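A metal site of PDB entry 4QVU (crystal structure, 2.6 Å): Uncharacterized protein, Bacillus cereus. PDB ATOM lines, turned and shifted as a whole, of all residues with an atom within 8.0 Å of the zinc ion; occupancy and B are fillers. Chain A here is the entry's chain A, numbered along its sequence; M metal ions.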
ATOM      1  N   ASN A 151      15.760 -13.891  -7.245  1.00  0.00           N
ATOM      2  CA  ASN A 151      14.877 -13.673  -6.095  1.00  0.00           C
ATOM      3  C   ASN A 151      13.713 -14.678  -6.194  1.00  0.00           C
ATOM      4  O   ASN A 151      13.726 -15.542  -7.081  1.00  0.00           O
ATOM      5  CB  ASN A 151      14.398 -12.214  -5.980  1.00  0.00           C
ATOM      6  CG  ASN A 151      13.662 -11.632  -7.166  1.00  0.00           C
ATOM      7  OD1 ASN A 151      12.806 -12.258  -7.790  1.00  0.00           O
ATOM      8  ND2 ASN A 151      13.917 -10.366  -7.441  1.00  0.00           N
ATOM      9  N   GLU A 152      12.725 -14.574  -5.299  1.00  0.00           N
ATOM     10  CA  GLU A 152      11.532 -15.447  -5.286  1.00  0.00           C
ATOM     11  C   GLU A 152      10.682 -15.304  -6.566  1.00  0.00           C
ATOM     12  O   GLU A 152      10.056 -16.276  -6.980  1.00  0.00           O
ATOM     13  CB  GLU A 152      10.654 -15.139  -4.054  1.00  0.00           C
ATOM     14  CG  GLU A 152      11.173 -15.691  -2.745  1.00  0.00           C
ATOM     15  CD  GLU A 152      10.240 -15.528  -1.555  1.00  0.00           C
ATOM     16  OE1 GLU A 152       9.309 -14.691  -1.641  1.00  0.00           O
ATOM     17  OE2 GLU A 152      10.452 -16.214  -0.528  1.00  0.00           O
ATOM     18  N   HIS A 153      10.646 -14.092  -7.172  1.00  0.00           N
ATOM     19  CA  HIS A 153       9.841 -13.769  -8.362  1.00  0.00           C
ATOM     20  C   HIS A 153      10.508 -14.145  -9.698  1.00  0.00           C
ATOM     21  O   HIS A 153       9.834 -14.681 -10.576  1.00  0.00           O
ATOM     22  CB  HIS A 153       9.537 -12.267  -8.415  1.00  0.00           C
ATOM     23  CG  HIS A 153       8.829 -11.726  -7.220  1.00  0.00           C
ATOM     24  ND1 HIS A 153       7.443 -11.748  -7.135  1.00  0.00           N
ATOM     25  CD2 HIS A 153       9.324 -11.088  -6.134  1.00  0.00           C
ATOM     26  CE1 HIS A 153       7.151 -11.167  -5.986  1.00  0.00           C
ATOM     27  NE2 HIS A 153       8.248 -10.751  -5.346  1.00  0.00           N
ATOM     28  N   ILE A 154      11.803 -13.777  -9.875  1.00  0.00           N
ATOM     29  CA  ILE A 154      12.518 -13.941 -11.146  1.00  0.00           C
ATOM     30  C   ILE A 154      13.968 -14.425 -10.942  1.00  0.00           C
ATOM     31  O   ILE A 154      14.564 -14.276  -9.868  1.00  0.00           O
ATOM     32  CB  ILE A 154      12.481 -12.566 -11.904  1.00  0.00           C
ATOM     33  CG1 ILE A 154      12.824 -12.713 -13.411  1.00  0.00           C
ATOM     34  CG2 ILE A 154      13.296 -11.476 -11.184  1.00  0.00           C
ATOM     35  CD1 ILE A 154      12.397 -11.586 -14.265  1.00  0.00           C
ATOM     36  N   ILE A 173      10.502 -16.784 -14.850  1.00  0.00           N
ATOM     37  CA  ILE A 173       9.474 -16.394 -13.873  1.00  0.00           C
ATOM     38  C   ILE A 173       8.641 -17.648 -13.596  1.00  0.00           C
ATOM     39  O   ILE A 173       8.490 -18.488 -14.480  1.00  0.00           O
ATOM     40  CB  ILE A 173       8.594 -15.156 -14.229  1.00  0.00           C
ATOM     41  CG1 ILE A 173       7.811 -15.335 -15.562  1.00  0.00           C
ATOM     42  CG2 ILE A 173       9.413 -13.865 -14.208  1.00  0.00           C
ATOM     43  CD1 ILE A 173       6.723 -14.319 -15.841  1.00  0.00           C
ATOM     44  N   GLU A 174       8.155 -17.798 -12.355  1.00  0.00           N
ATOM     45  CA  GLU A 174       7.394 -18.975 -11.946  1.00  0.00           C
ATOM     46  C   GLU A 174       5.893 -18.667 -11.903  1.00  0.00           C
ATOM     47  O   GLU A 174       5.077 -19.601 -11.960  1.00  0.00           O
ATOM     48  CB  GLU A 174       7.901 -19.472 -10.579  1.00  0.00           C
ATOM     49  CG  GLU A 174       7.730 -20.963 -10.368  1.00  0.00           C
ATOM     50  CD  GLU A 174       8.580 -21.518  -9.239  1.00  0.00           C
ATOM     51  OE1 GLU A 174       9.814 -21.642  -9.443  1.00  0.00           O
ATOM     52  OE2 GLU A 174       8.022 -21.834  -8.162  1.00  0.00           O
ATOM     53  N   ASP A 175       5.522 -17.369 -11.839  1.00  0.00           N
ATOM     54  CA  ASP A 175       4.129 -16.894 -11.821  1.00  0.00           C
ATOM     55  C   ASP A 175       3.935 -15.830 -12.911  1.00  0.00           C
ATOM     56  O   ASP A 175       4.815 -15.001 -13.137  1.00  0.00           O
ATOM     57  CB  ASP A 175       3.768 -16.345 -10.434  1.00  0.00           C
ATOM     58  CG  ASP A 175       2.320 -15.916 -10.281  1.00  0.00           C
ATOM     59  OD1 ASP A 175       1.454 -16.806 -10.121  1.00  0.00           O
ATOM     60  OD2 ASP A 175       2.067 -14.698 -10.266  1.00  0.00           O
ATOM     61  N   ILE A 176       2.746 -15.832 -13.556  1.00  0.00           N
ATOM     62  CA  ILE A 176       2.349 -14.909 -14.630  1.00  0.00           C
ATOM     63  C   ILE A 176       2.303 -13.446 -14.117  1.00  0.00           C
ATOM     64  O   ILE A 176       2.525 -12.533 -14.904  1.00  0.00           O
ATOM     65  CB  ILE A 176       0.978 -15.307 -15.265  1.00  0.00           C
ATOM     66  CG1 ILE A 176       0.767 -16.846 -15.271  1.00  0.00           C
ATOM     67  CG2 ILE A 176       0.828 -14.705 -16.680  1.00  0.00           C
ATOM     68  CD1 ILE A 176      -0.707 -17.324 -15.392  1.00  0.00           C
ATOM     69  N   GLY A 177       2.051 -13.247 -12.812  1.00  0.00           N
ATOM     70  CA  GLY A 177       2.021 -11.920 -12.181  1.00  0.00           C
ATOM     71  C   GLY A 177       3.340 -11.169 -12.199  1.00  0.00           C
ATOM     72  O   GLY A 177       3.352  -9.950 -12.014  1.00  0.00           O
ATOM     73  N   CYS A 178       4.473 -11.881 -12.444  1.00  0.00           N
ATOM     74  CA  CYS A 178       5.846 -11.340 -12.500  1.00  0.00           C
ATOM     75  C   CYS A 178       6.227 -10.966 -13.954  1.00  0.00           C
ATOM     76  O   CYS A 178       7.420 -10.823 -14.250  1.00  0.00           O
ATOM     77  CB  CYS A 178       6.832 -12.343 -11.931  1.00  0.00           C
ATOM     78  SG  CYS A 178       6.342 -13.056 -10.345  1.00  0.00           S
ATOM     79  N   ILE A 179       5.232 -10.804 -14.847  1.00  0.00           N
ATOM     80  CA  ILE A 179       5.421 -10.492 -16.270  1.00  0.00           C
ATOM     81  C   ILE A 179       6.091  -9.097 -16.458  1.00  0.00           C
ATOM     82  O   ILE A 179       6.906  -8.966 -17.373  1.00  0.00           O
ATOM     83  CB  ILE A 179       4.065 -10.599 -17.028  1.00  0.00           C
ATOM     84  CG1 ILE A 179       4.269 -10.544 -18.555  1.00  0.00           C
ATOM     85  CG2 ILE A 179       2.962  -9.628 -16.488  1.00  0.00           C
ATOM     86  CD1 ILE A 179       3.149 -11.099 -19.354  1.00  0.00           C
ATOM     87  N   ASP A 180       5.786  -8.098 -15.593  1.00  0.00           N
ATOM     88  CA  ASP A 180       6.401  -6.773 -15.678  1.00  0.00           C
ATOM     89  C   ASP A 180       7.883  -6.821 -15.265  1.00  0.00           C
ATOM     90  O   ASP A 180       8.686  -6.019 -15.739  1.00  0.00           O
ATOM     91  CB  ASP A 180       5.638  -5.761 -14.835  1.00  0.00           C
ATOM     92  CG  ASP A 180       4.236  -5.433 -15.335  1.00  0.00           C
ATOM     93  OD1 ASP A 180       3.964  -5.663 -16.541  1.00  0.00           O
ATOM     94  OD2 ASP A 180       3.444  -4.862 -14.543  1.00  0.00           O
ATOM     95  N   GLU A 181       8.249  -7.791 -14.409  1.00  0.00           N
ATOM     96  CA  GLU A 181       9.631  -7.996 -13.978  1.00  0.00           C
ATOM     97  C   GLU A 181      10.414  -8.616 -15.110  1.00  0.00           C
ATOM     98  O   GLU A 181      11.552  -8.232 -15.329  1.00  0.00           O
ATOM     99  CB  GLU A 181       9.701  -8.854 -12.709  1.00  0.00           C
ATOM    100  CG  GLU A 181       9.070  -8.198 -11.499  1.00  0.00           C
ATOM    101  CD  GLU A 181       9.108  -9.044 -10.241  1.00  0.00           C
ATOM    102  OE1 GLU A 181      10.187  -9.132  -9.604  1.00  0.00           O
ATOM    103  OE2 GLU A 181       8.042  -9.590  -9.870  1.00  0.00           O
ATOM    104  N   LEU A 182       9.780  -9.559 -15.864  1.00  0.00           N
ATOM    105  CA  LEU A 182      10.335 -10.242 -17.041  1.00  0.00           C
ATOM    106  C   LEU A 182      10.671  -9.198 -18.116  1.00  0.00           C
ATOM    107  O   LEU A 182      11.813  -9.142 -18.561  1.00  0.00           O
ATOM    108  CB  LEU A 182       9.329 -11.302 -17.561  1.00  0.00           C
ATOM    109  CG  LEU A 182       9.708 -12.141 -18.800  1.00  0.00           C
ATOM    110  CD1 LEU A 182      10.830 -13.093 -18.495  1.00  0.00           C
ATOM    111  CD2 LEU A 182       8.512 -12.957 -19.273  1.00  0.00           C
HETATM  112 ZN    ZN M   1       6.775 -11.012  -9.195  1.00  0.00          ZN
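The backbone NH (N) of His 153 lies within hydrogen-bond range of the side-chain amide oxygen (OD1) of Asn 151 (2.9 Å). The backbone carbonyl oxygen of Asp 175 lies close to the side-chain sulfur of Cys 178 (3.7 Å).
Three residues have an atom within 4 Å of the zinc ion: His 153, Cys 178 and Glu 181. Along chain A the residues within 4 Å of the zinc ion span positions 153 to 181. The nearest printed residue that does not touch the zinc ion is Gly 177 (4.6 Å).
The zinc ion is bound by OE2 of Glu 181. The zinc ion is bound by ND1 of His 153 (2.3 Å). SG of Cys 178 is bound to the zinc ion, at 2.4 Å. The zinc ion has three donor atoms within binding distance.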
